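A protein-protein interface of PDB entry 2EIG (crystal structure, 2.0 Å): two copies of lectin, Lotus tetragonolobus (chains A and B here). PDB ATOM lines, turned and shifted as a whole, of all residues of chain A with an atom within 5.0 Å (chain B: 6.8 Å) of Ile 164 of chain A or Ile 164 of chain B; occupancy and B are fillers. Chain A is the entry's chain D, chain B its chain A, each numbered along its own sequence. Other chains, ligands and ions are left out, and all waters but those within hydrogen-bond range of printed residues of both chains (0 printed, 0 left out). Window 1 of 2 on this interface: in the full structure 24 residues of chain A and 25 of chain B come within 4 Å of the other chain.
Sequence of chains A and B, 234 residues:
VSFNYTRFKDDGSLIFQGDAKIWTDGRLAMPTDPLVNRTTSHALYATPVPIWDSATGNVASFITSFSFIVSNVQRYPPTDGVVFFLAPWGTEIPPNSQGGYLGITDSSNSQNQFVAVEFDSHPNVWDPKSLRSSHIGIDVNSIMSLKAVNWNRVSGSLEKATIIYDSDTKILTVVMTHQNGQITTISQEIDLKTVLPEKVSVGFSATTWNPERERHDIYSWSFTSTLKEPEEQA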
ATOM      1  N   PHE A  62     -33.104 -23.639  25.564  1.00  0.00           N
ATOM      2  CA  PHE A  62     -34.128 -23.114  26.433  1.00  0.00           C
ATOM      3  C   PHE A  62     -33.610 -21.898  27.226  1.00  0.00           C
ATOM      4  O   PHE A  62     -32.413 -21.638  27.316  1.00  0.00           O
ATOM      5  CB  PHE A  62     -34.703 -24.211  27.358  1.00  0.00           C
ATOM      6  CG  PHE A  62     -33.738 -24.710  28.396  1.00  0.00           C
ATOM      7  CD1 PHE A  62     -33.498 -23.971  29.547  1.00  0.00           C
ATOM      8  CD2 PHE A  62     -33.045 -25.905  28.199  1.00  0.00           C
ATOM      9  CE1 PHE A  62     -32.588 -24.425  30.494  1.00  0.00           C
ATOM     10  CE2 PHE A  62     -32.126 -26.364  29.156  1.00  0.00           C
ATOM     11  CZ  PHE A  62     -31.908 -25.637  30.280  1.00  0.00           C
ATOM     12  N   ILE A  63     -34.534 -21.153  27.787  1.00  0.00           N
ATOM     13  CA  ILE A  63     -34.206 -20.171  28.781  1.00  0.00           C
ATOM     14  C   ILE A  63     -35.215 -20.349  29.856  1.00  0.00           C
ATOM     15  O   ILE A  63     -36.387 -20.652  29.615  1.00  0.00           O
ATOM     16  CB  ILE A  63     -34.211 -18.685  28.232  1.00  0.00           C
ATOM     17  CG1 ILE A  63     -34.124 -17.658  29.409  1.00  0.00           C
ATOM     18  CG2 ILE A  63     -35.439 -18.459  27.405  1.00  0.00           C
ATOM     19  CD1 ILE A  63     -33.811 -16.196  28.984  1.00  0.00           C
ATOM     20  N   THR A 162     -31.352 -16.310  35.758  1.00  0.00           N
ATOM     21  CA  THR A 162     -31.683 -16.614  34.392  1.00  0.00           C
ATOM     22  C   THR A 162     -30.703 -17.658  33.944  1.00  0.00           C
ATOM     23  O   THR A 162     -29.489 -17.537  34.158  1.00  0.00           O
ATOM     24  CB  THR A 162     -31.605 -15.395  33.483  1.00  0.00           C
ATOM     25  OG1 THR A 162     -32.459 -14.386  34.010  1.00  0.00           O
ATOM     26  CG2 THR A 162     -32.102 -15.740  32.062  1.00  0.00           C
ATOM     27  N   ILE A 163     -31.236 -18.685  33.304  1.00  0.00           N
ATOM     28  CA  ILE A 163     -30.414 -19.765  32.759  1.00  0.00           C
ATOM     29  C   ILE A 163     -30.724 -19.949  31.272  1.00  0.00           C
ATOM     30  O   ILE A 163     -31.884 -20.109  30.862  1.00  0.00           O
ATOM     31  CB  ILE A 163     -30.642 -21.109  33.521  1.00  0.00           C
ATOM     32  CG1 ILE A 163     -30.351 -20.946  35.022  1.00  0.00           C
ATOM     33  CG2 ILE A 163     -29.809 -22.248  32.849  1.00  0.00           C
ATOM     34  CD1 ILE A 163     -30.970 -22.071  35.970  1.00  0.00           C
ATOM     35  N   ILE A 164     -29.685 -19.948  30.462  1.00  0.00           N
ATOM     36  CA  ILE A 164     -29.897 -20.141  29.038  1.00  0.00           C
ATOM     37  C   ILE A 164     -29.087 -21.329  28.646  1.00  0.00           C
ATOM     38  O   ILE A 164     -27.883 -21.392  28.931  1.00  0.00           O
ATOM     39  CB  ILE A 164     -29.457 -18.922  28.135  1.00  0.00           C
ATOM     40  CG1 ILE A 164     -30.253 -17.648  28.491  1.00  0.00           C
ATOM     41  CG2 ILE A 164     -29.593 -19.289  26.606  1.00  0.00           C
ATOM     42  CD1 ILE A 164     -29.705 -16.335  27.896  1.00  0.00           C
ATOM     43  N   TYR A 165     -29.740 -22.244  27.952  1.00  0.00           N
ATOM     44  CA  TYR A 165     -29.025 -23.328  27.286  1.00  0.00           C
ATOM     45  C   TYR A 165     -29.067 -23.140  25.795  1.00  0.00           C
ATOM     46  O   TYR A 165     -30.128 -23.136  25.202  1.00  0.00           O
ATOM     47  CB  TYR A 165     -29.617 -24.702  27.608  1.00  0.00           C
ATOM     48  CG  TYR A 165     -28.819 -25.801  26.961  1.00  0.00           C
ATOM     49  CD1 TYR A 165     -27.594 -26.162  27.493  1.00  0.00           C
ATOM     50  CD2 TYR A 165     -29.268 -26.460  25.788  1.00  0.00           C
ATOM     51  CE1 TYR A 165     -26.822 -27.148  26.916  1.00  0.00           C
ATOM     52  CE2 TYR A 165     -28.458 -27.478  25.174  1.00  0.00           C
ATOM     53  CZ  TYR A 165     -27.239 -27.800  25.771  1.00  0.00           C
ATOM     54  OH  TYR A 165     -26.387 -28.769  25.298  1.00  0.00           O
ATOM     55  N   ASP A 166     -27.897 -22.966  25.199  1.00  0.00           N
ATOM     56  CA  ASP A 166     -27.810 -22.800  23.767  1.00  0.00           C
ATOM     57  C   ASP A 166     -27.381 -24.147  23.210  1.00  0.00           C
ATOM     58  O   ASP A 166     -26.234 -24.540  23.402  1.00  0.00           O
ATOM     59  CB  ASP A 166     -26.771 -21.736  23.395  1.00  0.00           C
ATOM     60  CG  ASP A 166     -26.537 -21.651  21.886  1.00  0.00           C
ATOM     61  OD1 ASP A 166     -27.517 -21.403  21.157  1.00  0.00           O
ATOM     62  OD2 ASP A 166     -25.379 -21.852  21.421  1.00  0.00           O
ATOM     63  N   ILE A 171     -23.865 -24.679  25.313  1.00  0.00           N
ATOM     64  CA  ILE A 171     -23.487 -23.994  26.529  1.00  0.00           C
ATOM     65  C   ILE A 171     -24.698 -23.749  27.413  1.00  0.00           C
ATOM     66  O   ILE A 171     -25.752 -23.317  26.952  1.00  0.00           O
ATOM     67  CB  ILE A 171     -22.655 -22.704  26.236  1.00  0.00           C
ATOM     68  CG1 ILE A 171     -21.213 -23.095  25.871  1.00  0.00           C
ATOM     69  CG2 ILE A 171     -22.653 -21.748  27.468  1.00  0.00           C
ATOM     70  CD1 ILE A 171     -20.617 -22.316  24.680  1.00  0.00           C
ATOM     71  N   LEU A 172     -24.527 -24.078  28.692  1.00  0.00           N
ATOM     72  CA  LEU A 172     -25.462 -23.691  29.721  1.00  0.00           C
ATOM     73  C   LEU A 172     -24.878 -22.484  30.435  1.00  0.00           C
ATOM     74  O   LEU A 172     -23.800 -22.563  30.950  1.00  0.00           O
ATOM     75  CB  LEU A 172     -25.618 -24.814  30.730  1.00  0.00           C
ATOM     76  CG  LEU A 172     -26.689 -24.579  31.792  1.00  0.00           C
ATOM     77  CD1 LEU A 172     -28.063 -24.735  31.143  1.00  0.00           C
ATOM     78  CD2 LEU A 172     -26.527 -25.583  32.878  1.00  0.00           C
ATOM     79  N   THR A 173     -25.582 -21.370  30.461  1.00  0.00           N
ATOM     80  CA  THR A 173     -25.044 -20.189  31.100  1.00  0.00           C
ATOM     81  C   THR A 173     -26.028 -19.668  32.098  1.00  0.00           C
ATOM     82  O   THR A 173     -27.218 -19.632  31.820  1.00  0.00           O
ATOM     83  CB  THR A 173     -24.759 -19.053  30.088  1.00  0.00           C
ATOM     84  OG1 THR A 173     -23.991 -19.569  29.009  1.00  0.00           O
ATOM     85  CG2 THR A 173     -23.947 -17.970  30.727  1.00  0.00           C
ATOM     86  N   VAL A 174     -25.513 -19.233  33.249  1.00  0.00           N
ATOM     87  CA  VAL A 174     -26.375 -18.778  34.341  1.00  0.00           C
ATOM     88  C   VAL A 174     -26.006 -17.366  34.687  1.00  0.00           C
ATOM     89  O   VAL A 174     -24.845 -17.042  34.790  1.00  0.00           O
ATOM     90  CB  VAL A 174     -26.161 -19.641  35.593  1.00  0.00           C
ATOM     91  CG1 VAL A 174     -27.131 -19.212  36.758  1.00  0.00           C
ATOM     92  CG2 VAL A 174     -26.280 -21.124  35.214  1.00  0.00           C
ATOM     93  N   VAL A 175     -27.002 -16.535  34.889  1.00  0.00           N
ATOM     94  CA  VAL A 175     -26.799 -15.246  35.521  1.00  0.00           C
ATOM     95  C   VAL A 175     -27.781 -15.084  36.677  1.00  0.00           C
ATOM     96  O   VAL A 175     -28.952 -15.492  36.569  1.00  0.00           O
ATOM     97  CB  VAL A 175     -26.961 -14.118  34.543  1.00  0.00           C
ATOM     98  CG1 VAL A 175     -28.344 -13.681  34.509  1.00  0.00           C
ATOM     99  CG2 VAL A 175     -26.167 -12.970  35.017  1.00  0.00           C
ATOM    100  N   THR A 185     -22.296 -14.787  37.300  1.00  0.00           N
ATOM    101  CA  THR A 185     -22.493 -15.653  36.159  1.00  0.00           C
ATOM    102  C   THR A 185     -21.599 -16.860  36.283  1.00  0.00           C
ATOM    103  O   THR A 185     -20.532 -16.816  36.892  1.00  0.00           O
ATOM    104  CB  THR A 185     -22.155 -14.985  34.822  1.00  0.00           C
ATOM    105  OG1 THR A 185     -20.806 -14.443  34.840  1.00  0.00           O
ATOM    106  CG2 THR A 185     -23.134 -13.952  34.477  1.00  0.00           C
ATOM    107  N   SER B  61     -19.038  -9.271  34.023  1.00  0.00           N
ATOM    108  CA  SER B  61     -20.153 -10.071  33.543  1.00  0.00           C
ATOM    109  C   SER B  61     -21.328  -9.155  33.388  1.00  0.00           C
ATOM    110  O   SER B  61     -21.454  -8.134  34.082  1.00  0.00           O
ATOM    111  CB  SER B  61     -20.516 -11.206  34.523  1.00  0.00           C
ATOM    112  OG  SER B  61     -19.504 -12.178  34.477  1.00  0.00           O
ATOM    113  N   PHE B  62     -22.229  -9.501  32.476  1.00  0.00           N
ATOM    114  CA  PHE B  62     -23.473  -8.779  32.445  1.00  0.00           C
ATOM    115  C   PHE B  62     -24.616  -9.667  32.028  1.00  0.00           C
ATOM    116  O   PHE B  62     -24.430 -10.761  31.461  1.00  0.00           O
ATOM    117  CB  PHE B  62     -23.412  -7.483  31.604  1.00  0.00           C
ATOM    118  CG  PHE B  62     -23.187  -7.689  30.101  1.00  0.00           C
ATOM    119  CD1 PHE B  62     -24.255  -7.968  29.246  1.00  0.00           C
ATOM    120  CD2 PHE B  62     -21.918  -7.542  29.563  1.00  0.00           C
ATOM    121  CE1 PHE B  62     -24.058  -8.140  27.862  1.00  0.00           C
ATOM    122  CE2 PHE B  62     -21.697  -7.722  28.189  1.00  0.00           C
ATOM    123  CZ  PHE B  62     -22.780  -8.014  27.340  1.00  0.00           C
ATOM    124  N   ILE B  63     -25.801  -9.182  32.328  1.00  0.00           N
ATOM    125  CA  ILE B  63     -26.984  -9.710  31.719  1.00  0.00           C
ATOM    126  C   ILE B  63     -27.758  -8.519  31.266  1.00  0.00           C
ATOM    127  O   ILE B  63     -27.842  -7.545  31.954  1.00  0.00           O
ATOM    128  CB  ILE B  63     -27.830 -10.620  32.667  1.00  0.00           C
ATOM    129  CG1 ILE B  63     -29.090 -11.105  31.924  1.00  0.00           C
ATOM    130  CG2 ILE B  63     -28.164  -9.889  34.031  1.00  0.00           C
ATOM    131  CD1 ILE B  63     -29.839 -12.244  32.600  1.00  0.00           C
ATOM    132  N   THR B  64     -28.291  -8.593  30.066  1.00  0.00           N
ATOM    133  CA  THR B  64     -29.182  -7.567  29.649  1.00  0.00           C
ATOM    134  C   THR B  64     -30.442  -8.228  29.085  1.00  0.00           C
ATOM    135  O   THR B  64     -30.342  -9.320  28.507  1.00  0.00           O
ATOM    136  CB  THR B  64     -28.490  -6.592  28.647  1.00  0.00           C
ATOM    137  OG1 THR B  64     -29.301  -5.460  28.524  1.00  0.00           O
ATOM    138  CG2 THR B  64     -28.238  -7.164  27.219  1.00  0.00           C
ATOM    139  N   THR B 162     -32.769 -11.856  25.830  1.00  0.00           N
ATOM    140  CA  THR B 162     -31.866 -11.880  26.961  1.00  0.00           C
ATOM    141  C   THR B 162     -30.446 -12.222  26.479  1.00  0.00           C
ATOM    142  O   THR B 162     -30.208 -13.172  25.720  1.00  0.00           O
ATOM    143  CB  THR B 162     -32.345 -12.925  27.997  1.00  0.00           C
ATOM    144  OG1 THR B 162     -33.677 -12.633  28.364  1.00  0.00           O
ATOM    145  CG2 THR B 162     -31.434 -12.988  29.221  1.00  0.00           C
ATOM    146  N   ILE B 163     -29.491 -11.436  26.933  1.00  0.00           N
ATOM    147  CA  ILE B 163     -28.097 -11.645  26.574  1.00  0.00           C
ATOM    148  C   ILE B 163     -27.302 -11.765  27.853  1.00  0.00           C
ATOM    149  O   ILE B 163     -27.423 -10.944  28.782  1.00  0.00           O
ATOM    150  CB  ILE B 163     -27.588 -10.480  25.708  1.00  0.00           C
ATOM    151  CG1 ILE B 163     -28.392 -10.386  24.377  1.00  0.00           C
ATOM    152  CG2 ILE B 163     -26.061 -10.593  25.454  1.00  0.00           C
ATOM    153  CD1 ILE B 163     -28.183  -9.064  23.659  1.00  0.00           C
ATOM    154  N   ILE B 164     -26.523 -12.817  27.959  1.00  0.00           N
ATOM    155  CA  ILE B 164     -25.745 -12.979  29.187  1.00  0.00           C
ATOM    156  C   ILE B 164     -24.326 -13.012  28.689  1.00  0.00           C
ATOM    157  O   ILE B 164     -24.050 -13.713  27.737  1.00  0.00           O
ATOM    158  CB  ILE B 164     -26.055 -14.286  29.968  1.00  0.00           C
ATOM    159  CG1 ILE B 164     -27.463 -14.258  30.570  1.00  0.00           C
ATOM    160  CG2 ILE B 164     -25.029 -14.504  31.115  1.00  0.00           C
ATOM    161  CD1 ILE B 164     -27.903 -15.607  31.203  1.00  0.00           C
ATOM    162  N   TYR B 165     -23.461 -12.200  29.289  1.00  0.00           N
ATOM    163  CA  TYR B 165     -22.031 -12.387  29.143  1.00  0.00           C
ATOM    164  C   TYR B 165     -21.457 -12.941  30.419  1.00  0.00           C
ATOM    165  O   TYR B 165     -21.453 -12.275  31.447  1.00  0.00           O
ATOM    166  CB  TYR B 165     -21.329 -11.072  28.769  1.00  0.00           C
ATOM    167  CG  TYR B 165     -19.865 -11.313  28.428  1.00  0.00           C
ATOM    168  CD1 TYR B 165     -19.491 -11.907  27.221  1.00  0.00           C
ATOM    169  CD2 TYR B 165     -18.874 -11.009  29.346  1.00  0.00           C
ATOM    170  CE1 TYR B 165     -18.162 -12.179  26.961  1.00  0.00           C
ATOM    171  CE2 TYR B 165     -17.548 -11.239  29.087  1.00  0.00           C
ATOM    172  CZ  TYR B 165     -17.194 -11.819  27.906  1.00  0.00           C
ATOM    173  OH  TYR B 165     -15.863 -12.018  27.699  1.00  0.00           O
ATOM    174  N   ASP B 166     -20.906 -14.130  30.345  1.00  0.00           N
ATOM    175  CA  ASP B 166     -20.232 -14.696  31.498  1.00  0.00           C
ATOM    176  C   ASP B 166     -18.713 -14.474  31.403  1.00  0.00           C
ATOM    177  O   ASP B 166     -18.067 -15.124  30.617  1.00  0.00           O
ATOM    178  CB  ASP B 166     -20.560 -16.184  31.625  1.00  0.00           C
ATOM    179  CG  ASP B 166     -19.732 -16.858  32.706  1.00  0.00           C
ATOM    180  OD1 ASP B 166     -19.430 -16.191  33.691  1.00  0.00           O
ATOM    181  OD2 ASP B 166     -19.365 -18.028  32.557  1.00  0.00           O
ATOM    182  N   ILE B 171     -18.177 -16.177  27.571  1.00  0.00           N
ATOM    183  CA  ILE B 171     -19.181 -16.555  26.582  1.00  0.00           C
ATOM    184  C   ILE B 171     -20.322 -15.547  26.605  1.00  0.00           C
ATOM    185  O   ILE B 171     -20.870 -15.247  27.651  1.00  0.00           O
ATOM    186  CB  ILE B 171     -19.683 -18.041  26.795  1.00  0.00           C
ATOM    187  CG1 ILE B 171     -18.531 -19.032  26.473  1.00  0.00           C
ATOM    188  CG2 ILE B 171     -20.862 -18.356  25.862  1.00  0.00           C
ATOM    189  CD1 ILE B 171     -18.618 -20.366  27.173  1.00  0.00           C
ATOM    190  N   LEU B 172     -20.635 -15.006  25.444  1.00  0.00           N
ATOM    191  CA  LEU B 172     -21.832 -14.198  25.238  1.00  0.00           C
ATOM    192  C   LEU B 172     -22.948 -15.097  24.694  1.00  0.00           C
ATOM    193  O   LEU B 172     -22.777 -15.719  23.660  1.00  0.00           O
ATOM    194  CB  LEU B 172     -21.514 -13.063  24.262  1.00  0.00           C
ATOM    195  CG  LEU B 172     -22.633 -12.056  23.931  1.00  0.00           C
ATOM    196  CD1 LEU B 172     -22.749 -11.098  25.068  1.00  0.00           C
ATOM    197  CD2 LEU B 172     -22.329 -11.307  22.646  1.00  0.00           C
ATOM    198  N   THR B 173     -24.091 -15.143  25.373  1.00  0.00           N
ATOM    199  CA  THR B 173     -25.187 -16.003  24.941  1.00  0.00           C
ATOM    200  C   THR B 173     -26.454 -15.194  24.825  1.00  0.00           C
ATOM    201  O   THR B 173     -26.799 -14.389  25.694  1.00  0.00           O
ATOM    202  CB  THR B 173     -25.389 -17.171  25.909  1.00  0.00           C
ATOM    203  OG1 THR B 173     -24.161 -17.873  26.003  1.00  0.00           O
ATOM    204  CG2 THR B 173     -26.436 -18.169  25.383  1.00  0.00           C
ATOM    205  N   VAL B 174     -27.167 -15.440  23.745  1.00  0.00           N
ATOM    206  CA  VAL B 174     -28.414 -14.780  23.529  1.00  0.00           C
ATOM    207  C   VAL B 174     -29.560 -15.783  23.574  1.00  0.00           C
ATOM    208  O   VAL B 174     -29.470 -16.852  22.984  1.00  0.00           O
ATOM    209  CB  VAL B 174     -28.427 -14.062  22.156  1.00  0.00           C
ATOM    210  CG1 VAL B 174     -29.663 -13.188  22.042  1.00  0.00           C
ATOM    211  CG2 VAL B 174     -27.089 -13.300  21.944  1.00  0.00           C
ATOM    212  N   VAL B 175     -30.630 -15.405  24.247  1.00  0.00           N
ATOM    213  CA  VAL B 175     -31.917 -16.020  23.993  1.00  0.00           C
ATOM    214  C   VAL B 175     -32.943 -14.986  23.508  1.00  0.00           C
ATOM    215  O   VAL B 175     -32.943 -13.845  24.008  1.00  0.00           O
ATOM    216  CB  VAL B 175     -32.398 -16.816  25.225  1.00  0.00           C
ATOM    217  CG1 VAL B 175     -32.391 -15.981  26.446  1.00  0.00           C
ATOM    218  CG2 VAL B 175     -33.777 -17.295  25.016  1.00  0.00           C
ATOM    219  N   THR B 184     -35.090 -18.771  20.337  1.00  0.00           N
ATOM    220  CA  THR B 184     -33.964 -18.930  19.468  1.00  0.00           C
ATOM    221  C   THR B 184     -32.786 -18.562  20.346  1.00  0.00           C
ATOM    222  O   THR B 184     -32.855 -17.606  21.151  1.00  0.00           O
ATOM    223  CB  THR B 184     -33.981 -17.911  18.328  1.00  0.00           C
ATOM    224  OG1 THR B 184     -35.078 -18.144  17.446  1.00  0.00           O
ATOM    225  CG2 THR B 184     -32.725 -18.014  17.535  1.00  0.00           C
ATOM    226  N   THR B 185     -31.696 -19.294  20.233  1.00  0.00           N
ATOM    227  CA  THR B 185     -30.521 -18.928  21.020  1.00  0.00           C
ATOM    228  C   THR B 185     -29.368 -18.953  20.072  1.00  0.00           C
ATOM    229  O   THR B 185     -29.398 -19.618  19.021  1.00  0.00           O
ATOM    230  CB  THR B 185     -30.211 -19.910  22.192  1.00  0.00           C
ATOM    231  OG1 THR B 185     -29.962 -21.231  21.656  1.00  0.00           O
ATOM    232  CG2 THR B 185     -31.359 -19.911  23.233  1.00  0.00           C
ATOM    233  N   ILE B 186     -28.347 -18.217  20.474  1.00  0.00           N
ATOM    234  CA  ILE B 186     -27.082 -18.211  19.783  1.00  0.00           C
ATOM    235  C   ILE B 186     -26.062 -17.781  20.830  1.00  0.00           C
ATOM    236  O   ILE B 186     -26.385 -17.101  21.833  1.00  0.00           O
ATOM    237  CB  ILE B 186     -27.175 -17.411  18.469  1.00  0.00           C
ATOM    238  CG1 ILE B 186     -25.926 -17.585  17.614  1.00  0.00           C
ATOM    239  CG2 ILE B 186     -27.595 -15.959  18.688  1.00  0.00           C
ATOM    240  CD1 ILE B 186     -24.969 -16.478  17.761  1.00  0.00           C
ATOM    241  N   SER B 187     -24.840 -18.279  20.660  1.00  0.00           N
ATOM    242  CA  SER B 187     -23.856 -18.133  21.696  1.00  0.00           C
ATOM    243  C   SER B 187     -22.462 -18.066  21.055  1.00  0.00           C
ATOM    244  O   SER B 187     -22.227 -18.619  19.967  1.00  0.00           O
ATOM    245  CB  SER B 187     -24.032 -19.237  22.747  1.00  0.00           C
ATOM    246  OG  SER B 187     -23.132 -19.085  23.813  1.00  0.00           O
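OD1 of Asp 166 of chain A sits at hydrogen-bond distance from OG1 of Thr 185 of chain B, 2.5 Å away.
The backbone NH (N) of Ile 186 of chain B lies within hydrogen-bond range of the side-chain carboxylate (OD1) of Asp 166 of chain A (3.4 Å).
The side-chain carboxylate of Asp 166 of chain B is in hydrogen-bond range of the side-chain hydroxyl of Thr 185 of chain A.
The side-chain hydroxyl (OG) of Ser 61 of chain B sits at hydrogen-bond distance from the side-chain hydroxyl (OG1) of Thr 185 of chain A (2.6 Å).
The side-chain hydroxyl (OG1) of Thr 173 of chain B sits at hydrogen-bond distance from the side-chain hydroxyl (OG1) of Thr 173 of chain A, at 3.5 Å.
The backbone NH of Thr 162 of chain B sits at hydrogen-bond distance from the backbone carbonyl oxygen of Val 175 of chain B, 2.7 Å away.
The backbone NH (N) of Tyr 165 of chain B sits at hydrogen-bond distance from the backbone carbonyl oxygen (O) of Phe 62 of chain B, 2.8 Å away.
The side-chain hydroxyl (OG1) of Thr 173 of chain B is in hydrogen-bond range of the side-chain hydroxyl (OG) of Ser 187 of chain B (2.7 Å).
O of Val 175 of chain A lies within hydrogen-bond range of N of Thr 162 of chain A (2.7 Å).
The backbone carbonyl oxygen of Ile 164 of chain A sits at hydrogen-bond distance from the backbone NH of Thr 173 of chain A, 2.8 Å away.
The backbone carbonyl oxygen (O) of Leu 172 of chain B sits close to the side-chain hydroxyl (OG) of Ser 187 of chain B (3.4 Å).
Thr 162 of chain B touches Ile 63 of chain A.
Ile 63 of chain A touches Val 175 of chain B.
O of Thr 162 of chain A touches CD1 of Ile 164 of chain B (3.9 Å).
Ile 164 of chain A touches Thr 162 of chain B.
CD1 of Ile 164 of chain B touches CD1 of Ile 164 of chain A, at 3.8 Å.
CG2 of Thr 173 of chain B touches CG2 of Ile 164 of chain A, at 3.6 Å.
Ile 164 of chain A touches Val 175 of chain B (CD1 to CG1, 3.1 Å).
CG2 of Thr 185 of chain B touches CG2 of Ile 164 of chain A (3.9 Å).
Thr 185 of chain B touches Tyr 165 of chain A (CG2 to O, 3.97 Å).
CG2 of Thr 185 of chain A touches O of Tyr 165 of chain B (3.8 Å).
Printed residues of chain B within 4 Å of Ile 63 of chain A: Thr 162 (3.6 Å) and Val 175 (2.9 Å).
Ile 164 of chain A touches just these residues of chain B: Thr 162, Ile 164, Thr 173, Val 175 and Thr 185.
Of the printed residues of chain B, Tyr 165 of chain A touches Thr 185.
Of the printed residues of chain B, Val 175 of chain A touches Ile 63 (2.8 Å) and Ile 164 (3.8 Å).
Of the printed residues of chain A, Ile 186 of chain B touches Asp 166.
The nearest residue of chain A that does not touch Ile 164 of chain B is Val 174 of chain A (4.3 Å).
The nearest printed residue of chain A that does not touch Asp 166 of chain B is Val 174 of chain A (5.4 Å).
Printed residues of chain A that touch a printed residue of chain B: Ile 63, Thr 162, Ile 164, Tyr 165, Asp 166, Ile 171, Thr 173, Val 175 and Thr 185.
Hydrophobic or aromatic side chains of chain A that line the printed part of chain B: Ile 63, Ile 164, Ile 171 and Val 175.
Along chain A the printed residues that touch a printed residue of chain B span positions 63 to 185.
Of the 18 printed residues of chain B, 12 touch a printed residue of chain A.
Printed residues of chain B that touch a printed residue of chain A: Ser 61, Ile 63, Thr 162, Ile 164, Tyr 165, Asp 166, Ile 171, Thr 173, Val 175, Thr 185, Ile 186 and Ser 187.
Hydrophobic or aromatic side chains of chain B within 4 Å of the printed part of chain A: Ile 63, Ile 164, Ile 171 and Val 175.
Ile 63 of chain A touches Val 175 of chain B, and with the chains exchanged Val 175 of chain A touches Ile 63 of chain B.
Ile 164 of chain A touches Thr 173 of chain B, and with the chains exchanged Thr 173 of chain A touches Ile 164 of chain B.
Asp 166 of chain A touches Thr 185 of chain B, and with the chains exchanged Thr 185 of chain A touches Asp 166 of chain B.
Thr 173 of chain B touches its own counterpart, Thr 173 of chain A.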
